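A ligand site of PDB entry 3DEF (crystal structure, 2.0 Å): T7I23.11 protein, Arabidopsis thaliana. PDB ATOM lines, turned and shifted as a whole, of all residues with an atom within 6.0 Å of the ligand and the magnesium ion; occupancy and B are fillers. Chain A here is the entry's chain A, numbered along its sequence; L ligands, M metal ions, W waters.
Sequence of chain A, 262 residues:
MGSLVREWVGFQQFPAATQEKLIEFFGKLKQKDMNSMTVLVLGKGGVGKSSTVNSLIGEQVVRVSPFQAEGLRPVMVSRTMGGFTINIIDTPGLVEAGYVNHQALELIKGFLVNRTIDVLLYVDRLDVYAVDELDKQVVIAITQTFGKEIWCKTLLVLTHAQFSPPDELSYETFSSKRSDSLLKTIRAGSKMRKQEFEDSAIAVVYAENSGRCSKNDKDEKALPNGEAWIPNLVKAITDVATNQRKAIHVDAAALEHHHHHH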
ATOM      1  N   LYS A  44      -5.565   1.547  24.709  1.00  0.00           N
ATOM      2  CA  LYS A  44      -5.341   2.505  23.678  1.00  0.00           C
ATOM      3  C   LYS A  44      -6.469   3.545  23.756  1.00  0.00           C
ATOM      4  O   LYS A  44      -7.478   3.277  24.332  1.00  0.00           O
ATOM      5  CB  LYS A  44      -5.379   1.788  22.333  1.00  0.00           C
ATOM      6  CG  LYS A  44      -4.247   0.737  22.162  1.00  0.00           C
ATOM      7  CD  LYS A  44      -4.248   0.102  20.746  1.00  0.00           C
ATOM      8  CE  LYS A  44      -5.474  -0.735  20.502  1.00  0.00           C
ATOM      9  NZ  LYS A  44      -5.385  -1.422  19.153  1.00  0.00           N
ATOM     10  N   GLY A  45      -6.307   4.715  23.169  1.00  0.00           N
ATOM     11  CA  GLY A  45      -7.418   5.673  23.042  1.00  0.00           C
ATOM     12  C   GLY A  45      -8.588   5.087  22.251  1.00  0.00           C
ATOM     13  O   GLY A  45      -8.422   4.310  21.352  1.00  0.00           O
ATOM     14  N   GLY A  46      -9.779   5.503  22.607  1.00  0.00           N
ATOM     15  CA  GLY A  46     -10.964   5.255  21.824  1.00  0.00           C
ATOM     16  C   GLY A  46     -11.502   3.855  21.911  1.00  0.00           C
ATOM     17  O   GLY A  46     -12.323   3.457  21.071  1.00  0.00           O
ATOM     18  N   VAL A  47     -11.137   3.106  22.938  1.00  0.00           N
ATOM     19  CA  VAL A  47     -11.622   1.728  23.051  1.00  0.00           C
ATOM     20  C   VAL A  47     -12.826   1.547  23.996  1.00  0.00           C
ATOM     21  O   VAL A  47     -13.346   0.452  24.067  1.00  0.00           O
ATOM     22  CB  VAL A  47     -10.498   0.731  23.514  1.00  0.00           C
ATOM     23  CG1 VAL A  47      -9.403   0.631  22.409  1.00  0.00           C
ATOM     24  CG2 VAL A  47      -9.875   1.119  24.882  1.00  0.00           C
ATOM     25  N   GLY A  48     -13.231   2.629  24.663  1.00  0.00           N
ATOM     26  CA  GLY A  48     -14.327   2.644  25.624  1.00  0.00           C
ATOM     27  C   GLY A  48     -13.917   2.459  27.093  1.00  0.00           C
ATOM     28  O   GLY A  48     -14.725   1.978  27.906  1.00  0.00           O
ATOM     29  N   LYS A  49     -12.710   2.879  27.463  1.00  0.00           N
ATOM     30  CA  LYS A  49     -12.306   2.847  28.873  1.00  0.00           C
ATOM     31  C   LYS A  49     -13.249   3.722  29.726  1.00  0.00           C
ATOM     32  O   LYS A  49     -13.857   3.258  30.661  1.00  0.00           O
ATOM     33  CB  LYS A  49     -10.844   3.375  29.039  1.00  0.00           C
ATOM     34  CG  LYS A  49      -9.810   2.489  28.337  1.00  0.00           C
ATOM     35  CD  LYS A  49      -8.360   2.990  28.583  1.00  0.00           C
ATOM     36  CE  LYS A  49      -8.087   4.375  28.124  1.00  0.00           C
ATOM     37  NZ  LYS A  49      -8.251   4.629  26.621  1.00  0.00           N
ATOM     38  N   SER A  50     -13.415   4.990  29.360  1.00  0.00           N
ATOM     39  CA  SER A  50     -14.261   5.879  30.154  1.00  0.00           C
ATOM     40  C   SER A  50     -15.714   5.432  30.147  1.00  0.00           C
ATOM     41  O   SER A  50     -16.436   5.542  31.178  1.00  0.00           O
ATOM     42  CB  SER A  50     -14.133   7.334  29.685  1.00  0.00           C
ATOM     43  OG  SER A  50     -12.804   7.794  29.812  1.00  0.00           O
ATOM     44  N   SER A  51     -16.194   5.004  28.993  1.00  0.00           N
ATOM     45  CA  SER A  51     -17.537   4.514  28.883  1.00  0.00           C
ATOM     46  C   SER A  51     -17.761   3.331  29.834  1.00  0.00           C
ATOM     47  O   SER A  51     -18.810   3.244  30.484  1.00  0.00           O
ATOM     48  CB  SER A  51     -17.907   4.145  27.456  1.00  0.00           C
ATOM     49  OG  SER A  51     -17.946   5.294  26.587  1.00  0.00           O
ATOM     50  N   THR A  52     -16.826   2.399  29.884  1.00  0.00           N
ATOM     51  CA  THR A  52     -16.952   1.230  30.777  1.00  0.00           C
ATOM     52  C   THR A  52     -16.912   1.627  32.265  1.00  0.00           C
ATOM     53  O   THR A  52     -17.670   1.098  33.124  1.00  0.00           O
ATOM     54  CB  THR A  52     -15.858   0.191  30.456  1.00  0.00           C
ATOM     55  OG1 THR A  52     -15.963  -0.137  29.083  1.00  0.00           O
ATOM     56  CG2 THR A  52     -16.027  -1.130  31.291  1.00  0.00           C
ATOM     57  N   ARG A  63     -15.337  11.663  31.352  1.00  0.00           N
ATOM     58  CA  ARG A  63     -15.726  12.239  30.075  1.00  0.00           C
ATOM     59  C   ARG A  63     -15.541  11.257  28.902  1.00  0.00           C
ATOM     60  O   ARG A  63     -14.461  10.721  28.710  1.00  0.00           O
ATOM     61  CB  ARG A  63     -14.864  13.458  29.813  1.00  0.00           C
ATOM     62  CG  ARG A  63     -15.216  14.151  28.561  1.00  0.00           C
ATOM     63  CD  ARG A  63     -14.818  15.623  28.678  1.00  0.00           C
ATOM     64  NE  ARG A  63     -13.645  15.947  27.906  1.00  0.00           N
ATOM     65  CZ  ARG A  63     -13.671  16.318  26.631  1.00  0.00           C
ATOM     66  NH1 ARG A  63     -14.820  16.438  25.966  1.00  0.00           N
ATOM     67  NH2 ARG A  63     -12.536  16.595  26.026  1.00  0.00           N
ATOM     68  N   VAL A  64     -16.573  11.063  28.104  1.00  0.00           N
ATOM     69  CA  VAL A  64     -16.538  10.161  26.950  1.00  0.00           C
ATOM     70  C   VAL A  64     -16.520  11.049  25.715  1.00  0.00           C
ATOM     71  O   VAL A  64     -17.184  12.082  25.702  1.00  0.00           O
ATOM     72  CB  VAL A  64     -17.789   9.266  26.954  1.00  0.00           C
ATOM     73  CG1 VAL A  64     -18.038   8.518  25.606  1.00  0.00           C
ATOM     74  CG2 VAL A  64     -17.686   8.265  28.067  1.00  0.00           C
ATOM     75  N   SER A  65     -15.783  10.637  24.685  1.00  0.00           N
ATOM     76  CA  SER A  65     -15.681  11.444  23.472  1.00  0.00           C
ATOM     77  C   SER A  65     -15.109  10.621  22.354  1.00  0.00           C
ATOM     78  O   SER A  65     -14.258   9.815  22.624  1.00  0.00           O
ATOM     79  CB  SER A  65     -14.733  12.606  23.684  1.00  0.00           C
ATOM     80  OG  SER A  65     -14.548  13.282  22.445  1.00  0.00           O
ATOM     81  N   PRO A  66     -15.524  10.875  21.108  1.00  0.00           N
ATOM     82  CA  PRO A  66     -14.863  10.212  20.011  1.00  0.00           C
ATOM     83  C   PRO A  66     -13.390  10.639  19.890  1.00  0.00           C
ATOM     84  O   PRO A  66     -12.579   9.916  19.336  1.00  0.00           O
ATOM     85  CB  PRO A  66     -15.696  10.632  18.785  1.00  0.00           C
ATOM     86  CG  PRO A  66     -16.422  11.778  19.183  1.00  0.00           C
ATOM     87  CD  PRO A  66     -16.601  11.756  20.627  1.00  0.00           C
ATOM     88  N   PHE A  67     -13.047  11.814  20.398  1.00  0.00           N
ATOM     89  CA  PHE A  67     -11.668  12.297  20.315  1.00  0.00           C
ATOM     90  C   PHE A  67     -10.973  12.205  21.634  1.00  0.00           C
ATOM     91  O   PHE A  67     -11.583  12.466  22.674  1.00  0.00           O
ATOM     92  CB  PHE A  67     -11.629  13.761  19.867  1.00  0.00           C
ATOM     93  CG  PHE A  67     -12.278  13.991  18.536  1.00  0.00           C
ATOM     94  CD1 PHE A  67     -11.605  13.676  17.366  1.00  0.00           C
ATOM     95  CD2 PHE A  67     -13.552  14.518  18.444  1.00  0.00           C
ATOM     96  CE1 PHE A  67     -12.219  13.886  16.134  1.00  0.00           C
ATOM     97  CE2 PHE A  67     -14.161  14.716  17.207  1.00  0.00           C
ATOM     98  CZ  PHE A  67     -13.494  14.410  16.065  1.00  0.00           C
ATOM     99  N   GLN A  68      -9.677  11.908  21.594  1.00  0.00           N
ATOM    100  CA  GLN A  68      -8.843  11.853  22.803  1.00  0.00           C
ATOM    101  C   GLN A  68      -8.543  13.294  23.197  1.00  0.00           C
ATOM    102  O   GLN A  68      -7.879  13.998  22.434  1.00  0.00           O
ATOM    103  CB  GLN A  68      -7.509  11.122  22.533  1.00  0.00           C
ATOM    104  CG  GLN A  68      -7.477  10.178  21.327  1.00  0.00           C
ATOM    105  CD  GLN A  68      -8.451   9.042  21.443  1.00  0.00           C
ATOM    106  OE1 GLN A  68      -8.677   8.532  22.537  1.00  0.00           O
ATOM    107  NE2 GLN A  68      -9.051   8.623  20.303  1.00  0.00           N
ATOM    108  N   ASP A  90      -9.300   5.802  35.843  1.00  0.00           N
ATOM    109  CA  ASP A  90      -9.399   5.987  34.407  1.00  0.00           C
ATOM    110  C   ASP A  90      -8.123   6.720  33.968  1.00  0.00           C
ATOM    111  O   ASP A  90      -7.484   7.433  34.779  1.00  0.00           O
ATOM    112  CB  ASP A  90     -10.650   6.762  34.051  1.00  0.00           C
ATOM    113  CG  ASP A  90     -11.006   6.728  32.576  1.00  0.00           C
ATOM    114  OD1 ASP A  90     -10.535   5.867  31.779  1.00  0.00           O
ATOM    115  OD2 ASP A  90     -11.803   7.620  32.172  1.00  0.00           O
ATOM    116  N   THR A  91      -7.769   6.493  32.714  1.00  0.00           N
ATOM    117  CA  THR A  91      -6.474   6.873  32.196  1.00  0.00           C
ATOM    118  C   THR A  91      -6.491   7.391  30.749  1.00  0.00           C
ATOM    119  O   THR A  91      -7.375   7.094  29.928  1.00  0.00           O
ATOM    120  CB  THR A  91      -5.482   5.659  32.271  1.00  0.00           C
ATOM    121  OG1 THR A  91      -6.023   4.580  31.531  1.00  0.00           O
ATOM    122  CG2 THR A  91      -5.232   5.195  33.740  1.00  0.00           C
ATOM    123  N   THR A 159     -15.009  -4.334  24.491  1.00  0.00           N
ATOM    124  CA  THR A 159     -16.149  -3.469  24.397  1.00  0.00           C
ATOM    125  C   THR A 159     -16.801  -3.718  23.012  1.00  0.00           C
ATOM    126  O   THR A 159     -16.296  -4.508  22.211  1.00  0.00           O
ATOM    127  CB  THR A 159     -15.813  -1.984  24.561  1.00  0.00           C
ATOM    128  OG1 THR A 159     -14.844  -1.618  23.562  1.00  0.00           O
ATOM    129  CG2 THR A 159     -15.154  -1.703  25.970  1.00  0.00           C
ATOM    130  N   HIS A 160     -17.903  -3.029  22.767  1.00  0.00           N
ATOM    131  CA  HIS A 160     -18.704  -3.206  21.499  1.00  0.00           C
ATOM    132  C   HIS A 160     -19.185  -4.628  21.338  1.00  0.00           C
ATOM    133  O   HIS A 160     -19.234  -5.182  20.208  1.00  0.00           O
ATOM    134  CB  HIS A 160     -17.862  -2.779  20.273  1.00  0.00           C
ATOM    135  CG  HIS A 160     -17.446  -1.350  20.257  1.00  0.00           C
ATOM    136  ND1 HIS A 160     -17.939  -0.455  19.329  1.00  0.00           N
ATOM    137  CD2 HIS A 160     -16.589  -0.651  21.033  1.00  0.00           C
ATOM    138  CE1 HIS A 160     -17.409   0.738  19.550  1.00  0.00           C
ATOM    139  NE2 HIS A 160     -16.571   0.638  20.571  1.00  0.00           N
ATOM    140  N   ALA A 161     -19.565  -5.267  22.451  1.00  0.00           N
ATOM    141  CA  ALA A 161     -19.897  -6.679  22.425  1.00  0.00           C
ATOM    142  C   ALA A 161     -21.135  -6.979  21.594  1.00  0.00           C
ATOM    143  O   ALA A 161     -21.280  -8.109  21.168  1.00  0.00           O
ATOM    144  CB  ALA A 161     -20.092  -7.242  23.831  1.00  0.00           C
ATOM    145  N   ALA A 207     -18.237  -6.388  27.152  1.00  0.00           N
ATOM    146  CA  ALA A 207     -18.996  -5.186  27.515  1.00  0.00           C
ATOM    147  C   ALA A 207     -19.640  -4.524  26.317  1.00  0.00           C
ATOM    148  O   ALA A 207     -19.081  -4.478  25.224  1.00  0.00           O
ATOM    149  CB  ALA A 207     -18.075  -4.194  28.180  1.00  0.00           C
ATOM    150  N   GLU A 208     -20.817  -3.923  26.544  1.00  0.00           N
ATOM    151  CA  GLU A 208     -21.480  -3.130  25.537  1.00  0.00           C
ATOM    152  C   GLU A 208     -22.008  -1.873  26.198  1.00  0.00           C
ATOM    153  O   GLU A 208     -22.999  -1.905  26.928  1.00  0.00           O
ATOM    154  CB  GLU A 208     -22.591  -3.954  24.832  1.00  0.00           C
ATOM    155  CG  GLU A 208     -23.318  -3.129  23.748  1.00  0.00           C
ATOM    156  CD  GLU A 208     -22.374  -2.467  22.769  1.00  0.00           C
ATOM    157  OE1 GLU A 208     -21.859  -3.180  21.871  1.00  0.00           O
ATOM    158  OE2 GLU A 208     -22.131  -1.253  22.880  1.00  0.00           O
ATOM    159  N   ASN A 209     -21.343  -0.766  25.940  1.00  0.00           N
ATOM    160  CA  ASN A 209     -21.677   0.490  26.558  1.00  0.00           C
ATOM    161  C   ASN A 209     -22.743   1.265  25.803  1.00  0.00           C
ATOM    162  O   ASN A 209     -23.192   2.291  26.285  1.00  0.00           O
ATOM    163  CB  ASN A 209     -20.443   1.341  26.714  1.00  0.00           C
ATOM    164  CG  ASN A 209     -19.382   0.721  27.655  1.00  0.00           C
ATOM    165  OD1 ASN A 209     -18.183   0.574  27.281  1.00  0.00           O
ATOM    166  ND2 ASN A 209     -19.788   0.419  28.871  1.00  0.00           N
ATOM    167  N   SER A 210     -23.118   0.810  24.625  1.00  0.00           N
ATOM    168  CA  SER A 210     -24.047   1.534  23.819  1.00  0.00           C
ATOM    169  C   SER A 210     -25.391   1.673  24.539  1.00  0.00           C
ATOM    170  O   SER A 210     -25.874   0.726  25.084  1.00  0.00           O
ATOM    171  CB  SER A 210     -24.286   0.809  22.498  1.00  0.00           C
ATOM    172  OG  SER A 210     -25.220   1.529  21.745  1.00  0.00           O
HETATM  173  P1  LIG L   1     -11.697   5.889  25.746  1.00  0.00           P
HETATM  174  O1  LIG L   1     -11.100   4.523  25.731  1.00  0.00           O
HETATM  175  O2  LIG L   1     -10.878   6.917  24.926  1.00  0.00           O
HETATM  176  O3  LIG L   1     -11.816   6.374  27.130  1.00  0.00           O
HETATM  177  O4  LIG L   1     -13.148   5.659  25.041  1.00  0.00           O
HETATM  178  P2  LIG L   1     -14.530   6.433  25.341  1.00  0.00           P
HETATM  179  O5  LIG L   1     -14.310   7.940  25.463  1.00  0.00           O
HETATM  180  O6  LIG L   1     -15.274   5.805  26.490  1.00  0.00           O
HETATM  181  O7  LIG L   1     -15.389   6.016  24.082  1.00  0.00           O
HETATM  182  C1  LIG L   1     -14.898   6.344  22.791  1.00  0.00           C
HETATM  183  C2  LIG L   1     -16.066   6.295  21.822  1.00  0.00           C
HETATM  184  O8  LIG L   1     -16.533   4.939  21.654  1.00  0.00           O
HETATM  185  C3  LIG L   1     -17.232   7.096  22.351  1.00  0.00           C
HETATM  186  O9  LIG L   1     -17.803   7.791  21.255  1.00  0.00           O
HETATM  187  C4  LIG L   1     -18.158   6.096  22.959  1.00  0.00           C
HETATM  188  O10 LIG L   1     -19.568   6.451  22.935  1.00  0.00           O
HETATM  189  C5  LIG L   1     -17.900   4.888  22.075  1.00  0.00           C
HETATM  190  N1  LIG L   1     -18.036   3.643  22.798  1.00  0.00           N
HETATM  191  C6  LIG L   1     -17.358   3.325  23.927  1.00  0.00           C
HETATM  192  N2  LIG L   1     -17.642   2.043  24.320  1.00  0.00           N
HETATM  193  C7  LIG L   1     -18.527   1.531  23.416  1.00  0.00           C
HETATM  194  C8  LIG L   1     -19.258   0.287  23.254  1.00  0.00           C
HETATM  195  O11 LIG L   1     -19.185  -0.678  24.093  1.00  0.00           O
HETATM  196  N3  LIG L   1     -20.095   0.226  22.177  1.00  0.00           N
HETATM  197  C9  LIG L   1     -20.260   1.233  21.305  1.00  0.00           C
HETATM  198  N4  LIG L   1     -21.073   1.044  20.251  1.00  0.00           N
HETATM  199  N5  LIG L   1     -19.599   2.395  21.381  1.00  0.00           N
HETATM  200  C10 LIG L   1     -18.797   2.618  22.443  1.00  0.00           C
HETATM  201 MG    MG M   1     -11.391   8.004  28.293  1.00  0.00          MG
HETATM  202  O   HOH W   1     -12.838   9.127  27.253  1.00  0.00           O
HETATM  203  O   HOH W   2     -20.248   5.733  25.504  1.00  0.00           O
HETATM  204  O   HOH W   3     -21.547  -1.795  19.700  1.00  0.00           O
HETATM  205  O   HOH W   4     -10.950   9.982  29.352  1.00  0.00           O
HETATM  206  O   HOH W   5      -9.925   8.544  26.747  1.00  0.00           O
HETATM  207  O   HOH W   6     -10.062   7.113  29.482  1.00  0.00           O
HETATM  208  O   HOH W   7     -14.953   2.651  21.440  1.00  0.00           O
HETATM  209  O   HOH W   8      -7.873   7.067  26.583  1.00  0.00           O
HETATM  210  O   HOH W   9     -19.403   9.956  22.102  1.00  0.00           O
HETATM  211  O   HOH W  10     -11.513   9.199  23.674  1.00  0.00           O
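Residues that only touch the magnesium ion: Asp 90 (3.9 Å).
Two residues have an atom within 4 Å of the magnesium ion: Ser 50 and Asp 90.
The backbone NH (N) of Phe 67 is in hydrogen-bond range of the side-chain hydroxyl (OG) of Ser 65.
OE2 of Glu 208 lies within hydrogen-bond range of N of Ser 210 (2.9 Å).
The side-chain amino group of Lys 49 sits at hydrogen-bond distance from the backbone carbonyl oxygen of Lys 44 (2.8 Å).
The side-chain hydroxyl of Thr 52 lies within hydrogen-bond range of the side-chain amide oxygen of Asn 209.
OG of Ser 50 lies close to OD2 of Asp 90 (2.6 Å).
The side-chain carboxylate (OE1) of Glu 208 lies within hydrogen-bond range of the backbone NH (N) of Ala 161, 3.2 Å away.
The backbone NH (N) of Gly 46 lies within hydrogen-bond range of the side-chain amide oxygen (OE1) of Gln 68, at 3.2 Å.
The backbone carbonyl oxygen (O) of Ala 207 lies within hydrogen-bond range of the backbone NH (N) of Ala 161, 2.9 Å away.
Water W1 bridges an oxygen (O5) of the ligand and the backbone carbonyl oxygen of Arg 63.
Water W6 bridges the side-chain carboxylate of Asp 90 (2.7 Å) and the backbone carbonyl oxygen of Thr 91 (2.7 Å).
Water W2 bridges the side-chain hydroxyl of Ser 51 (2.6 Å) and an oxygen (O10) of the ligand (2.8 Å).
Water W7 lies within hydrogen-bond range of NE2 of His 160 (2.7 Å), O of Gly 46 (2.8 Å) and O8 of the ligand (2.8 Å).
Water W3 bridges the side-chain carboxylate of Glu 208 (2.6 Å) and a nitrogen (N4) of the ligand (2.9 Å).
Water W8 lies within hydrogen-bond range of NZ of Lys 49 (2.5 Å), O of Thr 91 (3.4 Å) and O2 of the ligand (3.4 Å).
C of Gly 45 touches O2 of the ligand, at 3.97 Å.
Val 64 touches the ligand.
N of Pro 66 touches O9 of the ligand (3.8 Å).
Gln 68 touches the ligand.
Thr 159 touches the ligand (CB to O11, 3.6 Å).
Ala 207 touches the ligand (O to O11, 3.97 Å).
Ser 210 touches the ligand (CB to N4, 3.9 Å).
Hydrophobic or aromatic side chains that line the ligand: Val 47, Val 64 and His 160.
Of the 24 residues printed, 17 come within 4 Å of the ligand.
N of Val 47 sits at hydrogen-bond distance from O1 of the ligand, at 3.1 Å.
The backbone NH (N) of His 160 sits at hydrogen-bond distance from an oxygen (O11) of the ligand (3.0 Å).
O11 of the ligand sits at hydrogen-bond distance from N of Asn 209, at 2.8 Å.
The backbone NH of Ser 50 lies close to an oxygen (O3) of the ligand, at 3.1 Å.
OG of Ser 51 is in hydrogen-bond range of O6 of the ligand.
OE2 of Glu 208 lies within hydrogen-bond range of N3 of the ligand (2.6 Å).
The backbone NH (N) of Gly 48 sits at hydrogen-bond distance from an oxygen (O1) of the ligand, at 3.0 Å.
A nitrogen (N2) of the ligand lies close to the side-chain amide oxygen (OD1) of Asn 209 (3.3 Å).
N of Lys 49 lies within hydrogen-bond range of O1 of the ligand (2.9 Å).
N of Gly 46 lies within hydrogen-bond range of O2 of the ligand (2.9 Å).
O5 of the ligand sits at hydrogen-bond distance from N of Ser 65 (3.2 Å).
An oxygen (O6) of the ligand is in hydrogen-bond range of the backbone NH (N) of Ser 51, 2.8 Å away.
NZ of Lys 49 lies within salt-bridge range of O1 of the ligand (3.0 Å).
The magnesium ion is bound by water W6 (2.0 Å), O3 of the ligand (2.0 Å), OG of Ser 50 (2.1 Å), water W1 (2.1 Å), water W5 (2.2 Å) and water W4 (2.3 Å).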
